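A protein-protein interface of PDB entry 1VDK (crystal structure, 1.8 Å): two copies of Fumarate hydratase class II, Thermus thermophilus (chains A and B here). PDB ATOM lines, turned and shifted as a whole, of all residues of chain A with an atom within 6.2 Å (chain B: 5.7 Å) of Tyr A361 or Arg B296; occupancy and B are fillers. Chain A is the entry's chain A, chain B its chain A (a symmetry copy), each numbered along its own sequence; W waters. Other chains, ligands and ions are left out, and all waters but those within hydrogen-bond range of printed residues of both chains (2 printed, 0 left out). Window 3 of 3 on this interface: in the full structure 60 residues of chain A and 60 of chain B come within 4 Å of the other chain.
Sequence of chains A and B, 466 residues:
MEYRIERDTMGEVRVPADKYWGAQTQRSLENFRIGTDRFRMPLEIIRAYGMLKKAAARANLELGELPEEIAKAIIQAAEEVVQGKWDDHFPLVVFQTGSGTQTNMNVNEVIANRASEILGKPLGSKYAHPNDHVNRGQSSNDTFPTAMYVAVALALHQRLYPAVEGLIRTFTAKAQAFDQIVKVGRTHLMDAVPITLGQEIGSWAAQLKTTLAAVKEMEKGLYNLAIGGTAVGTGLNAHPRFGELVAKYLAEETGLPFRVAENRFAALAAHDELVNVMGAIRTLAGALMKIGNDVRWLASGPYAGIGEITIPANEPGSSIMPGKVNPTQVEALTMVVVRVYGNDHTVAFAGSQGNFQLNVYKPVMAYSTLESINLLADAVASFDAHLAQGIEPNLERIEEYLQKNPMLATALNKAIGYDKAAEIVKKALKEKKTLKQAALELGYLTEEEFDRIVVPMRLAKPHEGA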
ATOM      1  N   GLY A  98      -0.961  29.213   6.373  1.00  0.00           N
ATOM      2  CA  GLY A  98      -0.304  30.410   5.866  1.00  0.00           C
ATOM      3  C   GLY A  98      -1.220  31.497   5.341  1.00  0.00           C
ATOM      4  O   GLY A  98      -0.775  32.609   5.046  1.00  0.00           O
ATOM      5  N   SER A  99      -2.505  31.183   5.223  1.00  0.00           N
ATOM      6  CA  SER A  99      -3.483  32.152   4.732  1.00  0.00           C
ATOM      7  C   SER A  99      -4.227  32.798   5.894  1.00  0.00           C
ATOM      8  O   SER A  99      -4.959  33.773   5.707  1.00  0.00           O
ATOM      9  CB  SER A  99      -4.493  31.455   3.822  1.00  0.00           C
ATOM     10  OG  SER A  99      -5.160  30.426   4.536  1.00  0.00           O
ATOM     11  N   HIS A 271       2.862  40.814  -0.370  1.00  0.00           N
ATOM     12  CA  HIS A 271       2.600  41.875   0.590  1.00  0.00           C
ATOM     13  C   HIS A 271       3.845  42.736   0.622  1.00  0.00           C
ATOM     14  O   HIS A 271       4.402  43.027   1.676  1.00  0.00           O
ATOM     15  CB  HIS A 271       2.276  41.271   1.958  1.00  0.00           C
ATOM     16  CG  HIS A 271       1.061  40.402   1.925  1.00  0.00           C
ATOM     17  ND1 HIS A 271      -0.187  40.897   1.606  1.00  0.00           N
ATOM     18  CD2 HIS A 271       0.921  39.059   2.024  1.00  0.00           C
ATOM     19  CE1 HIS A 271      -1.040  39.893   1.500  1.00  0.00           C
ATOM     20  NE2 HIS A 271      -0.393  38.768   1.746  1.00  0.00           N
ATOM     21  N   ALA A 350      10.039  35.828   3.718  1.00  0.00           N
ATOM     22  CA  ALA A 350       8.682  35.341   3.473  1.00  0.00           C
ATOM     23  C   ALA A 350       8.033  36.065   2.291  1.00  0.00           C
ATOM     24  O   ALA A 350       7.290  35.464   1.512  1.00  0.00           O
ATOM     25  CB  ALA A 350       7.831  35.536   4.725  1.00  0.00           C
ATOM     26  N   GLY A 351       8.313  37.359   2.169  1.00  0.00           N
ATOM     27  CA  GLY A 351       7.730  38.144   1.092  1.00  0.00           C
ATOM     28  C   GLY A 351       8.121  37.701  -0.307  1.00  0.00           C
ATOM     29  O   GLY A 351       7.381  37.926  -1.264  1.00  0.00           O
ATOM     30  N   GLN A 353       8.553  34.594  -1.146  1.00  0.00           N
ATOM     31  CA  GLN A 353       8.084  33.225  -1.339  1.00  0.00           C
ATOM     32  C   GLN A 353       6.632  32.972  -1.745  1.00  0.00           C
ATOM     33  O   GLN A 353       6.136  31.851  -1.606  1.00  0.00           O
ATOM     34  CB  GLN A 353       8.412  32.432  -0.072  1.00  0.00           C
ATOM     35  CG  GLN A 353       9.896  32.484   0.300  1.00  0.00           C
ATOM     36  CD  GLN A 353      10.767  31.666  -0.645  1.00  0.00           C
ATOM     37  OE1 GLN A 353      10.693  30.436  -0.662  1.00  0.00           O
ATOM     38  NE2 GLN A 353      11.593  32.344  -1.435  1.00  0.00           N
ATOM     39  N   GLY A 354       5.944  33.991  -2.245  1.00  0.00           N
ATOM     40  CA  GLY A 354       4.568  33.777  -2.662  1.00  0.00           C
ATOM     41  C   GLY A 354       4.532  32.863  -3.876  1.00  0.00           C
ATOM     42  O   GLY A 354       5.505  32.783  -4.616  1.00  0.00           O
ATOM     43  N   ASN A 355       3.423  32.157  -4.074  1.00  0.00           N
ATOM     44  CA  ASN A 355       3.286  31.269  -5.226  1.00  0.00           C
ATOM     45  C   ASN A 355       1.934  31.487  -5.882  1.00  0.00           C
ATOM     46  O   ASN A 355       0.903  31.488  -5.215  1.00  0.00           O
ATOM     47  CB  ASN A 355       3.395  29.796  -4.819  1.00  0.00           C
ATOM     48  CG  ASN A 355       4.769  29.430  -4.291  1.00  0.00           C
ATOM     49  OD1 ASN A 355       4.916  29.087  -3.126  1.00  0.00           O
ATOM     50  ND2 ASN A 355       5.778  29.498  -5.152  1.00  0.00           N
ATOM     51  N   ASN A 359       0.224  34.343  -1.344  1.00  0.00           N
ATOM     52  CA  ASN A 359       1.440  34.236  -0.553  1.00  0.00           C
ATOM     53  C   ASN A 359       0.930  33.576   0.726  1.00  0.00           C
ATOM     54  O   ASN A 359       0.015  34.097   1.369  1.00  0.00           O
ATOM     55  CB  ASN A 359       2.021  35.618  -0.240  1.00  0.00           C
ATOM     56  CG  ASN A 359       3.167  35.553   0.752  1.00  0.00           C
ATOM     57  OD1 ASN A 359       2.987  35.124   1.891  1.00  0.00           O
ATOM     58  ND2 ASN A 359       4.354  35.970   0.322  1.00  0.00           N
ATOM     59  N   VAL A 360       1.478  32.417   1.078  1.00  0.00           N
ATOM     60  CA  VAL A 360       1.026  31.746   2.290  1.00  0.00           C
ATOM     61  C   VAL A 360       1.989  31.786   3.475  1.00  0.00           C
ATOM     62  O   VAL A 360       2.275  30.764   4.117  1.00  0.00           O
ATOM     63  CB  VAL A 360       0.577  30.289   2.008  1.00  0.00           C
ATOM     64  CG1 VAL A 360      -0.740  30.320   1.223  1.00  0.00           C
ATOM     65  CG2 VAL A 360       1.649  29.537   1.220  1.00  0.00           C
ATOM     66  N   TYR A 361       2.471  32.994   3.759  1.00  0.00           N
ATOM     67  CA  TYR A 361       3.344  33.273   4.899  1.00  0.00           C
ATOM     68  C   TYR A 361       2.747  34.486   5.618  1.00  0.00           C
ATOM     69  O   TYR A 361       3.429  35.147   6.398  1.00  0.00           O
ATOM     70  CB  TYR A 361       4.768  33.648   4.453  1.00  0.00           C
ATOM     71  CG  TYR A 361       5.597  32.501   3.925  1.00  0.00           C
ATOM     72  CD1 TYR A 361       5.454  32.054   2.610  1.00  0.00           C
ATOM     73  CD2 TYR A 361       6.500  31.835   4.754  1.00  0.00           C
ATOM     74  CE1 TYR A 361       6.188  30.967   2.137  1.00  0.00           C
ATOM     75  CE2 TYR A 361       7.235  30.743   4.293  1.00  0.00           C
ATOM     76  CZ  TYR A 361       7.073  30.314   2.987  1.00  0.00           C
ATOM     77  OH  TYR A 361       7.772  29.219   2.536  1.00  0.00           O
ATOM     78  N   LYS A 362       1.470  34.770   5.378  1.00  0.00           N
ATOM     79  CA  LYS A 362       0.859  35.961   5.967  1.00  0.00           C
ATOM     80  C   LYS A 362       0.980  36.147   7.478  1.00  0.00           C
ATOM     81  O   LYS A 362       1.407  37.209   7.937  1.00  0.00           O
ATOM     82  CB  LYS A 362      -0.619  36.071   5.554  1.00  0.00           C
ATOM     83  CG  LYS A 362      -0.861  35.940   4.049  1.00  0.00           C
ATOM     84  CD  LYS A 362      -2.287  36.360   3.678  1.00  0.00           C
ATOM     85  CE  LYS A 362      -2.647  35.941   2.246  1.00  0.00           C
ATOM     86  NZ  LYS A 362      -1.646  36.397   1.232  1.00  0.00           N
ATOM     87  N   PRO A 363       0.614  35.128   8.278  1.00  0.00           N
ATOM     88  CA  PRO A 363       0.717  35.299   9.729  1.00  0.00           C
ATOM     89  C   PRO A 363       2.091  35.700  10.260  1.00  0.00           C
ATOM     90  O   PRO A 363       2.201  36.612  11.082  1.00  0.00           O
ATOM     91  CB  PRO A 363       0.256  33.942  10.270  1.00  0.00           C
ATOM     92  CG  PRO A 363      -0.765  33.522   9.247  1.00  0.00           C
ATOM     93  CD  PRO A 363      -0.046  33.848   7.949  1.00  0.00           C
ATOM     94  N   VAL A 364       3.141  35.040   9.783  1.00  0.00           N
ATOM     95  CA  VAL A 364       4.469  35.351  10.282  1.00  0.00           C
ATOM     96  C   VAL A 364       4.963  36.715   9.793  1.00  0.00           C
ATOM     97  O   VAL A 364       5.702  37.394  10.501  1.00  0.00           O
ATOM     98  CB  VAL A 364       5.482  34.209   9.942  1.00  0.00           C
ATOM     99  CG1 VAL A 364       5.810  34.196   8.451  1.00  0.00           C
ATOM    100  CG2 VAL A 364       6.747  34.370  10.787  1.00  0.00           C
ATOM    101  N   MET A 365       4.543  37.132   8.601  1.00  0.00           N
ATOM    102  CA  MET A 365       4.947  38.445   8.094  1.00  0.00           C
ATOM    103  C   MET A 365       4.323  39.528   8.975  1.00  0.00           C
ATOM    104  O   MET A 365       4.984  40.491   9.361  1.00  0.00           O
ATOM    105  CB  MET A 365       4.489  38.626   6.641  1.00  0.00           C
ATOM    106  CG  MET A 365       5.249  37.755   5.654  1.00  0.00           C
ATOM    107  SD  MET A 365       4.731  38.011   3.943  1.00  0.00           S
ATOM    108  CE  MET A 365       5.590  39.538   3.550  1.00  0.00           C
ATOM    109  N   ALA A 366       3.044  39.358   9.297  1.00  0.00           N
ATOM    110  CA  ALA A 366       2.348  40.328  10.139  1.00  0.00           C
ATOM    111  C   ALA A 366       2.892  40.291  11.560  1.00  0.00           C
ATOM    112  O   ALA A 366       3.127  41.334  12.173  1.00  0.00           O
ATOM    113  CB  ALA A 366       0.854  40.037  10.150  1.00  0.00           C
ATOM    114  N   MET B 289      12.842  23.624   4.807  1.00  0.00           N
ATOM    115  CA  MET B 289      12.071  24.388   3.833  1.00  0.00           C
ATOM    116  C   MET B 289      12.126  23.667   2.482  1.00  0.00           C
ATOM    117  O   MET B 289      11.107  23.499   1.815  1.00  0.00           O
ATOM    118  CB  MET B 289      12.622  25.811   3.677  1.00  0.00           C
ATOM    119  CG  MET B 289      11.990  26.561   2.507  1.00  0.00           C
ATOM    120  SD  MET B 289      12.453  28.289   2.377  1.00  0.00           S
ATOM    121  CE  MET B 289      11.233  29.038   3.506  1.00  0.00           C
ATOM    122  N   ILE B 291      12.638  20.505   1.857  1.00  0.00           N
ATOM    123  CA  ILE B 291      11.816  19.304   1.984  1.00  0.00           C
ATOM    124  C   ILE B 291      10.328  19.654   1.996  1.00  0.00           C
ATOM    125  O   ILE B 291       9.529  19.056   1.270  1.00  0.00           O
ATOM    126  CB  ILE B 291      12.167  18.551   3.281  1.00  0.00           C
ATOM    127  CG1 ILE B 291      13.599  18.017   3.186  1.00  0.00           C
ATOM    128  CG2 ILE B 291      11.164  17.419   3.533  1.00  0.00           C
ATOM    129  CD1 ILE B 291      14.171  17.560   4.517  1.00  0.00           C
ATOM    130  N   GLY B 292       9.959  20.622   2.828  1.00  0.00           N
ATOM    131  CA  GLY B 292       8.567  21.025   2.910  1.00  0.00           C
ATOM    132  C   GLY B 292       8.030  21.479   1.565  1.00  0.00           C
ATOM    133  O   GLY B 292       6.913  21.132   1.182  1.00  0.00           O
ATOM    134  N   ASN B 293       8.818  22.265   0.842  1.00  0.00           N
ATOM    135  CA  ASN B 293       8.377  22.733  -0.464  1.00  0.00           C
ATOM    136  C   ASN B 293       8.227  21.567  -1.437  1.00  0.00           C
ATOM    137  O   ASN B 293       7.274  21.530  -2.216  1.00  0.00           O
ATOM    138  CB  ASN B 293       9.332  23.795  -1.013  1.00  0.00           C
ATOM    139  CG  ASN B 293       9.052  25.168  -0.431  1.00  0.00           C
ATOM    140  OD1 ASN B 293       7.915  25.468  -0.067  1.00  0.00           O
ATOM    141  ND2 ASN B 293      10.077  26.011  -0.351  1.00  0.00           N
ATOM    142  N   ASP B 294       9.153  20.610  -1.395  1.00  0.00           N
ATOM    143  CA  ASP B 294       9.043  19.442  -2.270  1.00  0.00           C
ATOM    144  C   ASP B 294       7.718  18.737  -1.973  1.00  0.00           C
ATOM    145  O   ASP B 294       6.984  18.347  -2.885  1.00  0.00           O
ATOM    146  CB  ASP B 294      10.189  18.455  -2.021  1.00  0.00           C
ATOM    147  CG  ASP B 294      11.414  18.744  -2.866  1.00  0.00           C
ATOM    148  OD1 ASP B 294      11.424  19.752  -3.602  1.00  0.00           O
ATOM    149  OD2 ASP B 294      12.375  17.949  -2.788  1.00  0.00           O
ATOM    150  N   VAL B 295       7.418  18.577  -0.689  1.00  0.00           N
ATOM    151  CA  VAL B 295       6.188  17.917  -0.269  1.00  0.00           C
ATOM    152  C   VAL B 295       4.926  18.600  -0.797  1.00  0.00           C
ATOM    153  O   VAL B 295       4.049  17.937  -1.357  1.00  0.00           O
ATOM    154  CB  VAL B 295       6.097  17.825   1.275  1.00  0.00           C
ATOM    155  CG1 VAL B 295       4.707  17.358   1.694  1.00  0.00           C
ATOM    156  CG2 VAL B 295       7.146  16.852   1.802  1.00  0.00           C
ATOM    157  N   ARG B 296       4.810  19.914  -0.628  1.00  0.00           N
ATOM    158  CA  ARG B 296       3.602  20.560  -1.123  1.00  0.00           C
ATOM    159  C   ARG B 296       3.539  20.630  -2.643  1.00  0.00           C
ATOM    160  O   ARG B 296       2.449  20.602  -3.220  1.00  0.00           O
ATOM    161  CB  ARG B 296       3.393  21.950  -0.498  1.00  0.00           C
ATOM    162  CG  ARG B 296       4.492  22.973  -0.677  1.00  0.00           C
ATOM    163  CD  ARG B 296       4.009  24.307  -0.084  1.00  0.00           C
ATOM    164  NE  ARG B 296       5.100  25.239   0.188  1.00  0.00           N
ATOM    165  CZ  ARG B 296       4.979  26.311   0.964  1.00  0.00           C
ATOM    166  NH1 ARG B 296       3.811  26.592   1.534  1.00  0.00           N
ATOM    167  NH2 ARG B 296       6.035  27.083   1.203  1.00  0.00           N
ATOM    168  N   TRP B 297       4.689  20.694  -3.308  1.00  0.00           N
ATOM    169  CA  TRP B 297       4.665  20.725  -4.762  1.00  0.00           C
ATOM    170  C   TRP B 297       4.268  19.348  -5.296  1.00  0.00           C
ATOM    171  O   TRP B 297       3.504  19.248  -6.252  1.00  0.00           O
ATOM    172  CB  TRP B 297       6.020  21.159  -5.335  1.00  0.00           C
ATOM    173  CG  TRP B 297       6.189  22.647  -5.360  1.00  0.00           C
ATOM    174  CD1 TRP B 297       7.003  23.396  -4.562  1.00  0.00           C
ATOM    175  CD2 TRP B 297       5.487  23.573  -6.201  1.00  0.00           C
ATOM    176  NE1 TRP B 297       6.852  24.735  -4.852  1.00  0.00           N
ATOM    177  CE2 TRP B 297       5.926  24.871  -5.853  1.00  0.00           C
ATOM    178  CE3 TRP B 297       4.530  23.432  -7.218  1.00  0.00           C
ATOM    179  CZ2 TRP B 297       5.440  26.024  -6.483  1.00  0.00           C
ATOM    180  CZ3 TRP B 297       4.046  24.580  -7.847  1.00  0.00           C
ATOM    181  CH2 TRP B 297       4.504  25.860  -7.474  1.00  0.00           C
ATOM    182  N   LEU B 298       4.767  18.288  -4.667  1.00  0.00           N
ATOM    183  CA  LEU B 298       4.427  16.938  -5.105  1.00  0.00           C
ATOM    184  C   LEU B 298       2.951  16.638  -4.868  1.00  0.00           C
ATOM    185  O   LEU B 298       2.336  15.875  -5.616  1.00  0.00           O
ATOM    186  CB  LEU B 298       5.289  15.904  -4.375  1.00  0.00           C
ATOM    187  CG  LEU B 298       6.748  15.847  -4.838  1.00  0.00           C
ATOM    188  CD1 LEU B 298       7.543  14.905  -3.945  1.00  0.00           C
ATOM    189  CD2 LEU B 298       6.799  15.387  -6.294  1.00  0.00           C
ATOM    190  N   ALA B 299       2.381  17.251  -3.835  1.00  0.00           N
ATOM    191  CA  ALA B 299       0.977  17.037  -3.512  1.00  0.00           C
ATOM    192  C   ALA B 299       0.061  18.081  -4.152  1.00  0.00           C
ATOM    193  O   ALA B 299      -1.158  18.021  -3.994  1.00  0.00           O
ATOM    194  CB  ALA B 299       0.790  17.040  -1.993  1.00  0.00           C
ATOM    195  N   SER B 300       0.645  19.025  -4.887  1.00  0.00           N
ATOM    196  CA  SER B 300      -0.135  20.086  -5.517  1.00  0.00           C
ATOM    197  C   SER B 300      -1.225  19.575  -6.448  1.00  0.00           C
ATOM    198  O   SER B 300      -1.095  18.519  -7.072  1.00  0.00           O
ATOM    199  CB  SER B 300       0.776  21.051  -6.284  1.00  0.00           C
ATOM    200  OG  SER B 300       1.410  20.419  -7.382  1.00  0.00           O
ATOM    201  N   PRO B 327      -1.863  21.990   2.070  1.00  0.00           N
ATOM    202  CA  PRO B 327      -0.718  21.489   2.846  1.00  0.00           C
ATOM    203  C   PRO B 327      -0.416  22.396   4.038  1.00  0.00           C
ATOM    204  O   PRO B 327       0.679  22.940   4.162  1.00  0.00           O
ATOM    205  CB  PRO B 327       0.405  21.490   1.819  1.00  0.00           C
ATOM    206  CG  PRO B 327       0.100  22.723   1.017  1.00  0.00           C
ATOM    207  CD  PRO B 327      -1.414  22.632   0.821  1.00  0.00           C
ATOM    208  N   VAL B 330       2.792  22.108   6.073  1.00  0.00           N
ATOM    209  CA  VAL B 330       3.981  22.607   5.380  1.00  0.00           C
ATOM    210  C   VAL B 330       4.063  24.119   5.582  1.00  0.00           C
ATOM    211  O   VAL B 330       5.143  24.687   5.759  1.00  0.00           O
ATOM    212  CB  VAL B 330       3.931  22.324   3.854  1.00  0.00           C
ATOM    213  CG1 VAL B 330       5.030  23.102   3.138  1.00  0.00           C
ATOM    214  CG2 VAL B 330       4.120  20.832   3.597  1.00  0.00           C
ATOM    215  N   GLU B 331       2.909  24.769   5.555  1.00  0.00           N
ATOM    216  CA  GLU B 331       2.867  26.211   5.732  1.00  0.00           C
ATOM    217  C   GLU B 331       3.336  26.612   7.127  1.00  0.00           C
ATOM    218  O   GLU B 331       4.107  27.556   7.275  1.00  0.00           O
ATOM    219  CB  GLU B 331       1.451  26.715   5.439  1.00  0.00           C
ATOM    220  CG  GLU B 331       1.132  26.656   3.942  1.00  0.00           C
ATOM    221  CD  GLU B 331      -0.348  26.761   3.631  1.00  0.00           C
ATOM    222  OE1 GLU B 331      -1.123  27.166   4.521  1.00  0.00           O
ATOM    223  OE2 GLU B 331      -0.731  26.441   2.483  1.00  0.00           O
ATOM    224  N   THR B 334       7.226  26.018   7.212  1.00  0.00           N
ATOM    225  CA  THR B 334       8.014  27.014   6.495  1.00  0.00           C
ATOM    226  C   THR B 334       7.937  28.407   7.129  1.00  0.00           C
ATOM    227  O   THR B 334       8.875  29.196   6.998  1.00  0.00           O
ATOM    228  CB  THR B 334       7.640  27.078   4.984  1.00  0.00           C
ATOM    229  OG1 THR B 334       6.228  27.256   4.828  1.00  0.00           O
ATOM    230  CG2 THR B 334       8.068  25.782   4.284  1.00  0.00           C
ATOM    231  N   MET B 335       6.838  28.717   7.815  1.00  0.00           N
ATOM    232  CA  MET B 335       6.752  30.008   8.488  1.00  0.00           C
ATOM    233  C   MET B 335       7.726  29.962   9.662  1.00  0.00           C
ATOM    234  O   MET B 335       8.364  30.960   9.992  1.00  0.00           O
ATOM    235  CB  MET B 335       5.321  30.312   8.960  1.00  0.00           C
ATOM    236  CG  MET B 335       4.410  30.742   7.810  1.00  0.00           C
ATOM    237  SD  MET B 335       2.934  31.657   8.325  1.00  0.00           S
ATOM    238  CE  MET B 335       1.945  30.317   9.006  1.00  0.00           C
ATOM    239  N   VAL B 338      11.279  30.616   8.178  1.00  0.00           N
ATOM    240  CA  VAL B 338      11.678  31.999   7.929  1.00  0.00           C
ATOM    241  C   VAL B 338      11.908  32.742   9.242  1.00  0.00           C
ATOM    242  O   VAL B 338      12.729  33.657   9.306  1.00  0.00           O
ATOM    243  CB  VAL B 338      10.664  32.762   7.021  1.00  0.00           C
ATOM    244  CG1 VAL B 338      10.624  32.096   5.657  1.00  0.00           C
ATOM    245  CG2 VAL B 338       9.282  32.801   7.646  1.00  0.00           C
HETATM  246  O   HOH W   1       8.763  28.775   0.218  1.00  0.00           O
HETATM  247  O   HOH W   2       4.087  28.556   3.674  1.00  0.00           O
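The backbone NH (N) of Val A364 is in hydrogen-bond range of the side-chain sulfur (SD) of Met B335 (3.7 Å).
OH of Tyr A361 sits close to OG1 of Thr B334 (3.4 Å).
OH of Tyr A361 lies within hydrogen-bond range of NH2 of Arg B296, 3.1 Å away.
N of Gly A98 lies within hydrogen-bond range of OE1 of Glu B331 (2.8 Å).
The side-chain amide oxygen (OD1) of Asn A355 sits close to the backbone carbonyl oxygen (O) of Gln A353 (3.4 Å).
O of Val B330 lies within hydrogen-bond range of OG1 of Thr B334.
The backbone carbonyl oxygen of Trp B297 lies within hydrogen-bond range of the side-chain hydroxyl of Ser B300 (2.7 Å).
The side-chain amide oxygen (OD1) of Asn A359 is in hydrogen-bond range of the backbone NH (N) of Tyr A361, at 2.9 Å.
N of Lys A362 sits at hydrogen-bond distance from O of Gly A98, at 3.1 Å.
The side-chain amide oxygen (OD1) of Asn B293 lies within hydrogen-bond range of the guanidinium group (NH2) of Arg B296 (2.8 Å).
Among the printed residues, pairs that only touch across the chains: Gly A98 with Met B335 (3.9 Å), Asn A355 with Trp B297 (3.7 Å), Val A360 with Arg B296 (3.7 Å), Val A360 with Glu B331 (3.99 Å), Tyr A361 with Met B289 (3.6 Å), Tyr A361 with Met B335 (3.8 Å), Tyr A361 with Val B338 (3.9 Å), Pro A363 with Met B335 (3.7 Å) and Val A364 with Val B338 (3.8 Å).
Arg B296 touches just these residues of chain A: Val A360 (3.7 Å) and Tyr A361 (3.1 Å).
Of the printed residues of chain B, Pro A363 touches Met B335.
Printed residues of chain A within 4 Å of Met B335: Gly A98 (3.9 Å), Tyr A361 (3.8 Å), Pro A363 (3.7 Å) and Val A364 (3.7 Å).
Printed residues of chain B within 4 Å of Val A360: Arg B296 (3.7 Å) and Glu B331 (3.99 Å).
Asn B293 touches none of the printed residues of chain A.
The nearest residue of chain B that does not touch Tyr A361 is Asn B293 (4.6 Å).
The nearest residue of chain A that does not touch Arg B296 is Asn A355 (4.9 Å).
Printed residues of chain B that touch a printed residue of chain A: Met B289, Arg B296, Trp B297, Glu B331, Thr B334, Met B335 and Val B338.
Hydrophobic or aromatic side chains of chain B within 4 Å of the printed part of chain A: Met B289, Trp B297, Met B335 and Val B338.
Printed residues of chain A that touch a printed residue of chain B: Gly A98, Asn A355, Val A360, Tyr A361, Pro A363 and Val A364.
Hydrophobic or aromatic side chains of chain A within 4 Å of the printed part of chain B: Val A360, Tyr A361, Pro A363 and Val A364.
No position is printed for both chains.
Of the 13 pairs that touch across the chains among the printed residues, none has its exchanged pair printed and touching as well.
Water W1 lies within hydrogen-bond range of OH of Tyr A361 (2.6 Å), OE1 of Gln A353 (2.7 Å), ND2 of Asn B293 (3.1 Å) and NH2 of Arg B296 (3.4 Å).
Water W2 lies within hydrogen-bond range of the side-chain hydroxyl (OG1) of Thr B334, the backbone carbonyl oxygen (O) of Val A360 and the guanidinium group (NH1) of Arg B296.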
